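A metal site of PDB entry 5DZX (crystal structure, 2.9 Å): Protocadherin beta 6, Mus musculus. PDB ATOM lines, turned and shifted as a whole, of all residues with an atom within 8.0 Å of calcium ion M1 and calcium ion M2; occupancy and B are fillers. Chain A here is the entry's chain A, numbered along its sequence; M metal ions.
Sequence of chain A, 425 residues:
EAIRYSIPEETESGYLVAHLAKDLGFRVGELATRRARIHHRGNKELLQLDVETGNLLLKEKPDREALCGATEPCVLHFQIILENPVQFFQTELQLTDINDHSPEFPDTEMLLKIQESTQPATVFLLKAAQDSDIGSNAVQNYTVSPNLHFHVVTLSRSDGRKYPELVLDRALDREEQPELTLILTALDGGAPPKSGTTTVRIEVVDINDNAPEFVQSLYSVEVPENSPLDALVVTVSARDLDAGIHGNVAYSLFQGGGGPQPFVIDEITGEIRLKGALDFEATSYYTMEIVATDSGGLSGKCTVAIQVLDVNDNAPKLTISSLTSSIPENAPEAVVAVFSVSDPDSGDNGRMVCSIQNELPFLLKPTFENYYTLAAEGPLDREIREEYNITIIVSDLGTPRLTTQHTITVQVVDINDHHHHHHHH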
ATOM      1  N   GLU A 116      25.048 -27.073 -29.708  1.00  0.00           N
ATOM      2  CA  GLU A 116      23.924 -26.676 -30.547  1.00  0.00           C
ATOM      3  C   GLU A 116      24.351 -26.399 -31.990  1.00  0.00           C
ATOM      4  O   GLU A 116      23.599 -26.666 -32.928  1.00  0.00           O
ATOM      5  CB  GLU A 116      23.260 -25.441 -29.941  1.00  0.00           C
ATOM      6  CG  GLU A 116      22.076 -24.874 -30.722  1.00  0.00           C
ATOM      7  CD  GLU A 116      21.571 -23.571 -30.121  1.00  0.00           C
ATOM      8  OE1 GLU A 116      22.113 -23.145 -29.085  1.00  0.00           O
ATOM      9  OE2 GLU A 116      20.633 -22.985 -30.695  1.00  0.00           O
ATOM     10  N   SER A 117      25.570 -25.911 -32.162  1.00  0.00           N
ATOM     11  CA  SER A 117      26.083 -25.516 -33.467  1.00  0.00           C
ATOM     12  C   SER A 117      26.707 -26.681 -34.235  1.00  0.00           C
ATOM     13  O   SER A 117      27.522 -26.479 -35.133  1.00  0.00           O
ATOM     14  CB  SER A 117      27.138 -24.413 -33.321  1.00  0.00           C
ATOM     15  OG  SER A 117      28.202 -24.842 -32.508  1.00  0.00           O
ATOM     16  N   LEU A 172      20.503 -29.515 -34.367  1.00  0.00           N
ATOM     17  CA  LEU A 172      20.003 -29.425 -32.992  1.00  0.00           C
ATOM     18  C   LEU A 172      19.779 -27.979 -32.558  1.00  0.00           C
ATOM     19  O   LEU A 172      20.479 -27.067 -33.003  1.00  0.00           O
ATOM     20  CB  LEU A 172      20.964 -30.104 -32.026  1.00  0.00           C
ATOM     21  CG  LEU A 172      21.194 -31.599 -32.221  1.00  0.00           C
ATOM     22  CD1 LEU A 172      22.274 -32.106 -31.272  1.00  0.00           C
ATOM     23  CD2 LEU A 172      19.900 -32.359 -32.003  1.00  0.00           C
ATOM     24  N   ASP A 173      18.794 -27.786 -31.681  1.00  0.00           N
ATOM     25  CA  ASP A 173      18.521 -26.483 -31.114  1.00  0.00           C
ATOM     26  C   ASP A 173      18.245 -26.608 -29.621  1.00  0.00           C
ATOM     27  O   ASP A 173      17.362 -27.364 -29.205  1.00  0.00           O
ATOM     28  CB  ASP A 173      17.326 -25.834 -31.808  1.00  0.00           C
ATOM     29  CG  ASP A 173      17.459 -24.326 -31.918  1.00  0.00           C
ATOM     30  OD1 ASP A 173      18.596 -23.837 -32.114  1.00  0.00           O
ATOM     31  OD2 ASP A 173      16.428 -23.627 -31.789  1.00  0.00           O
ATOM     32  N   ARG A 174      19.004 -25.871 -28.806  1.00  0.00           N
ATOM     33  CA  ARG A 174      18.866 -25.956 -27.363  1.00  0.00           C
ATOM     34  C   ARG A 174      17.601 -25.222 -26.906  1.00  0.00           C
ATOM     35  O   ARG A 174      17.005 -25.555 -25.876  1.00  0.00           O
ATOM     36  CB  ARG A 174      20.090 -25.370 -26.665  1.00  0.00           C
ATOM     37  CG  ARG A 174      20.036 -25.498 -25.152  1.00  0.00           C
ATOM     38  CD  ARG A 174      20.978 -24.536 -24.472  1.00  0.00           C
ATOM     39  NE  ARG A 174      20.391 -23.958 -23.275  1.00  0.00           N
ATOM     40  CZ  ARG A 174      19.752 -22.786 -23.250  1.00  0.00           C
ATOM     41  NH1 ARG A 174      19.637 -22.065 -24.350  1.00  0.00           N
ATOM     42  NH2 ARG A 174      19.235 -22.344 -22.105  1.00  0.00           N
ATOM     43  N   GLU A 175      17.205 -24.216 -27.680  1.00  0.00           N
ATOM     44  CA  GLU A 175      16.066 -23.383 -27.327  1.00  0.00           C
ATOM     45  C   GLU A 175      14.760 -24.172 -27.359  1.00  0.00           C
ATOM     46  O   GLU A 175      13.835 -23.884 -26.594  1.00  0.00           O
ATOM     47  CB  GLU A 175      15.984 -22.168 -28.250  1.00  0.00           C
ATOM     48  CG  GLU A 175      17.010 -21.084 -27.924  1.00  0.00           C
ATOM     49  CD  GLU A 175      18.442 -21.520 -28.161  1.00  0.00           C
ATOM     50  OE1 GLU A 175      18.663 -22.409 -29.018  1.00  0.00           O
ATOM     51  OE2 GLU A 175      19.352 -21.006 -27.479  1.00  0.00           O
ATOM     52  N   GLU A 176      14.684 -25.159 -28.244  1.00  0.00           N
ATOM     53  CA  GLU A 176      13.492 -25.993 -28.324  1.00  0.00           C
ATOM     54  C   GLU A 176      13.583 -27.193 -27.384  1.00  0.00           C
ATOM     55  O   GLU A 176      12.676 -27.442 -26.587  1.00  0.00           O
ATOM     56  CB  GLU A 176      13.263 -26.479 -29.762  1.00  0.00           C
ATOM     57  CG  GLU A 176      12.808 -25.390 -30.716  1.00  0.00           C
ATOM     58  CD  GLU A 176      12.502 -25.925 -32.094  1.00  0.00           C
ATOM     59  OE1 GLU A 176      12.046 -25.134 -32.951  1.00  0.00           O
ATOM     60  OE2 GLU A 176      12.705 -27.132 -32.329  1.00  0.00           O
ATOM     61  N   VAL A 204      22.602 -30.914 -24.978  1.00  0.00           N
ATOM     62  CA  VAL A 204      22.953 -29.860 -25.930  1.00  0.00           C
ATOM     63  C   VAL A 204      23.651 -28.710 -25.209  1.00  0.00           C
ATOM     64  O   VAL A 204      23.154 -28.198 -24.206  1.00  0.00           O
ATOM     65  CB  VAL A 204      21.712 -29.313 -26.657  1.00  0.00           C
ATOM     66  CG1 VAL A 204      22.149 -28.400 -27.797  1.00  0.00           C
ATOM     67  CG2 VAL A 204      20.866 -30.451 -27.198  1.00  0.00           C
ATOM     68  N   VAL A 205      24.800 -28.306 -25.738  1.00  0.00           N
ATOM     69  CA  VAL A 205      25.592 -27.229 -25.151  1.00  0.00           C
ATOM     70  C   VAL A 205      25.174 -25.878 -25.745  1.00  0.00           C
ATOM     71  O   VAL A 205      25.072 -25.739 -26.963  1.00  0.00           O
ATOM     72  CB  VAL A 205      27.100 -27.445 -25.370  1.00  0.00           C
ATOM     73  CG1 VAL A 205      27.911 -26.288 -24.814  1.00  0.00           C
ATOM     74  CG2 VAL A 205      27.535 -28.758 -24.731  1.00  0.00           C
ATOM     75  N   ASP A 206      24.933 -24.900 -24.882  1.00  0.00           N
ATOM     76  CA  ASP A 206      24.475 -23.583 -25.322  1.00  0.00           C
ATOM     77  C   ASP A 206      25.561 -22.853 -26.091  1.00  0.00           C
ATOM     78  O   ASP A 206      26.704 -22.757 -25.633  1.00  0.00           O
ATOM     79  CB  ASP A 206      24.031 -22.739 -24.123  1.00  0.00           C
ATOM     80  CG  ASP A 206      23.457 -21.389 -24.544  1.00  0.00           C
ATOM     81  OD1 ASP A 206      22.877 -21.308 -25.655  1.00  0.00           O
ATOM     82  OD2 ASP A 206      23.588 -20.415 -23.772  1.00  0.00           O
ATOM     83  N   ILE A 207      25.211 -22.368 -27.270  1.00  0.00           N
ATOM     84  CA  ILE A 207      26.105 -21.538 -28.051  1.00  0.00           C
ATOM     85  C   ILE A 207      25.434 -20.212 -28.360  1.00  0.00           C
ATOM     86  O   ILE A 207      24.236 -20.053 -28.154  1.00  0.00           O
ATOM     87  CB  ILE A 207      26.537 -22.238 -29.363  1.00  0.00           C
ATOM     88  CG1 ILE A 207      25.323 -22.514 -30.241  1.00  0.00           C
ATOM     89  CG2 ILE A 207      27.301 -23.520 -29.055  1.00  0.00           C
ATOM     90  CD1 ILE A 207      25.340 -21.736 -31.535  1.00  0.00           C
ATOM     91  N   ASN A 208      26.222 -19.268 -28.844  1.00  0.00           N
ATOM     92  CA  ASN A 208      25.719 -17.922 -29.095  1.00  0.00           C
ATOM     93  C   ASN A 208      25.151 -17.755 -30.502  1.00  0.00           C
ATOM     94  O   ASN A 208      25.872 -17.406 -31.435  1.00  0.00           O
ATOM     95  CB  ASN A 208      26.831 -16.914 -28.850  1.00  0.00           C
ATOM     96  CG  ASN A 208      26.301 -15.559 -28.473  1.00  0.00           C
ATOM     97  OD1 ASN A 208      25.198 -15.435 -27.946  1.00  0.00           O
ATOM     98  ND2 ASN A 208      27.094 -14.515 -28.722  1.00  0.00           N
ATOM     99  N   ASP A 209      23.847 -17.990 -30.642  1.00  0.00           N
ATOM    100  CA  ASP A 209      23.204 -17.913 -31.945  1.00  0.00           C
ATOM    101  C   ASP A 209      21.958 -17.028 -31.944  1.00  0.00           C
ATOM    102  O   ASP A 209      21.304 -16.845 -32.978  1.00  0.00           O
ATOM    103  CB  ASP A 209      22.854 -19.316 -32.446  1.00  0.00           C
ATOM    104  CG  ASP A 209      22.094 -20.125 -31.416  1.00  0.00           C
ATOM    105  OD1 ASP A 209      22.275 -19.883 -30.204  1.00  0.00           O
ATOM    106  OD2 ASP A 209      21.327 -21.030 -31.807  1.00  0.00           O
ATOM    107  N   ASN A 210      21.619 -16.466 -30.782  1.00  0.00           N
ATOM    108  CA  ASN A 210      20.472 -15.576 -30.667  1.00  0.00           C
ATOM    109  C   ASN A 210      20.853 -14.194 -30.160  1.00  0.00           C
ATOM    110  O   ASN A 210      21.340 -14.043 -29.040  1.00  0.00           O
ATOM    111  CB  ASN A 210      19.408 -16.189 -29.759  1.00  0.00           C
ATOM    112  CG  ASN A 210      18.746 -17.399 -30.370  1.00  0.00           C
ATOM    113  OD1 ASN A 210      18.583 -17.485 -31.588  1.00  0.00           O
ATOM    114  ND2 ASN A 210      18.378 -18.354 -29.525  1.00  0.00           N
ATOM    115  N   ASP A 240      17.470 -12.188 -23.725  1.00  0.00           N
ATOM    116  CA  ASP A 240      18.287 -13.061 -24.565  1.00  0.00           C
ATOM    117  C   ASP A 240      17.845 -14.510 -24.431  1.00  0.00           C
ATOM    118  O   ASP A 240      17.701 -15.028 -23.329  1.00  0.00           O
ATOM    119  CB  ASP A 240      19.765 -12.929 -24.204  1.00  0.00           C
ATOM    120  CG  ASP A 240      20.685 -13.362 -25.325  1.00  0.00           C
ATOM    121  OD1 ASP A 240      20.247 -14.162 -26.165  1.00  0.00           O
ATOM    122  OD2 ASP A 240      21.837 -12.897 -25.349  1.00  0.00           O
ATOM    123  N   LEU A 241      17.641 -15.154 -25.575  1.00  0.00           N
ATOM    124  CA  LEU A 241      17.200 -16.552 -25.599  1.00  0.00           C
ATOM    125  C   LEU A 241      18.262 -17.498 -25.059  1.00  0.00           C
ATOM    126  O   LEU A 241      17.943 -18.534 -24.473  1.00  0.00           O
ATOM    127  CB  LEU A 241      16.796 -16.964 -27.020  1.00  0.00           C
ATOM    128  CG  LEU A 241      15.547 -16.312 -27.611  1.00  0.00           C
ATOM    129  CD1 LEU A 241      15.292 -16.849 -29.009  1.00  0.00           C
ATOM    130  CD2 LEU A 241      14.341 -16.540 -26.708  1.00  0.00           C
ATOM    131  N   ASP A 242      19.531 -17.141 -25.270  1.00  0.00           N
ATOM    132  CA  ASP A 242      20.642 -17.984 -24.830  1.00  0.00           C
ATOM    133  C   ASP A 242      20.819 -17.932 -23.306  1.00  0.00           C
ATOM    134  O   ASP A 242      20.220 -17.099 -22.627  1.00  0.00           O
ATOM    135  CB  ASP A 242      21.926 -17.543 -25.521  1.00  0.00           C
ATOM    136  CG  ASP A 242      21.830 -17.598 -27.030  1.00  0.00           C
ATOM    137  OD1 ASP A 242      21.113 -18.486 -27.555  1.00  0.00           O
ATOM    138  OD2 ASP A 242      22.447 -16.751 -27.709  1.00  0.00           O
ATOM    139  N   ALA A 243      21.650 -18.824 -22.788  1.00  0.00           N
ATOM    140  CA  ALA A 243      21.885 -18.889 -21.346  1.00  0.00           C
ATOM    141  C   ALA A 243      23.365 -18.704 -21.031  1.00  0.00           C
ATOM    142  O   ALA A 243      24.210 -18.703 -21.928  1.00  0.00           O
ATOM    143  CB  ALA A 243      21.379 -20.197 -20.773  1.00  0.00           C
ATOM    144  N   HIS A 246      26.258 -16.299 -22.714  1.00  0.00           N
ATOM    145  CA  HIS A 246      25.635 -15.991 -23.989  1.00  0.00           C
ATOM    146  C   HIS A 246      24.271 -15.338 -23.772  1.00  0.00           C
ATOM    147  O   HIS A 246      23.636 -14.891 -24.730  1.00  0.00           O
ATOM    148  CB  HIS A 246      25.481 -17.252 -24.846  1.00  0.00           C
ATOM    149  CG  HIS A 246      26.709 -18.111 -24.886  1.00  0.00           C
ATOM    150  ND1 HIS A 246      27.863 -17.739 -25.546  1.00  0.00           N
ATOM    151  CD2 HIS A 246      26.954 -19.336 -24.372  1.00  0.00           C
ATOM    152  CE1 HIS A 246      28.770 -18.694 -25.426  1.00  0.00           C
ATOM    153  NE2 HIS A 246      28.242 -19.677 -24.712  1.00  0.00           N
HETATM  154 CA    CA M   1      19.131 -21.520 -31.235  1.00  0.00          CA
HETATM  155 CA    CA M   2      21.695 -21.066 -27.748  1.00  0.00          CA
HETATM  156 CA    CA M   3      22.816 -13.903 -27.148  1.00  0.00          CA
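Asn 210 touches calcium ion M1 (ND2 to CA, 3.7 Å). The nearest printed residue that does not touch calcium ion M1 is Arg 174 (5.0 Å).
OE2 of Glu 116 is bound to calcium ion M1 (2.2 Å). Calcium ion M1 is bound by OD2 of Asp 209, 2.3 Å away. OE1 of Glu 175 binds calcium ion M1. OD1 of Asp 173 binds calcium ion M1, 2.5 Å away. Calcium ion M1 has four donor atoms within binding distance.
Calcium ion M2 is bound by the side-chain carboxylate of Glu 175, the side-chain carboxylate of Asp 206, the side-chain carboxylate of Glu 116, the side-chain carboxylate of Asp 242, the backbone carbonyl oxygen of Ile 207 and the side-chain carboxylate of Asp 209. Calcium ion M2 has six donor atoms within binding distance.
OE2 of Glu 175 lies close to NH1 of Arg 174. The side-chain carboxylate (OD2) of Asp 242 lies within hydrogen-bond range of the backbone NH (N) of Asn 210 (3.2 Å). The side-chain carboxylate (OD2) of Asp 206 sits at hydrogen-bond distance from the backbone NH (N) of Ala 243 (2.7 Å). OD1 of Asp 206 lies close to NH1 of Arg 174, at 3.6 Å. The backbone NH (N) of Asp 242 sits close to the side-chain carboxylate (OD1) of Asp 240 (3.2 Å). O of Val 205 sits at hydrogen-bond distance from N of Glu 116. OE2 of Glu 175 lies close to ND2 of Asn 210. The side-chain carboxylate (OD2) of Asp 242 lies close to the side-chain amide oxygen (OD1) of Asn 208 (3.1 Å).
Six residues have an atom within 4 Å of calcium ion M2: Glu 116, Glu 175, Asp 206, Ile 207, Asp 209 and Asp 242. The nearest printed residue that does not touch calcium ion M2 is Arg 174 (4.1 Å).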
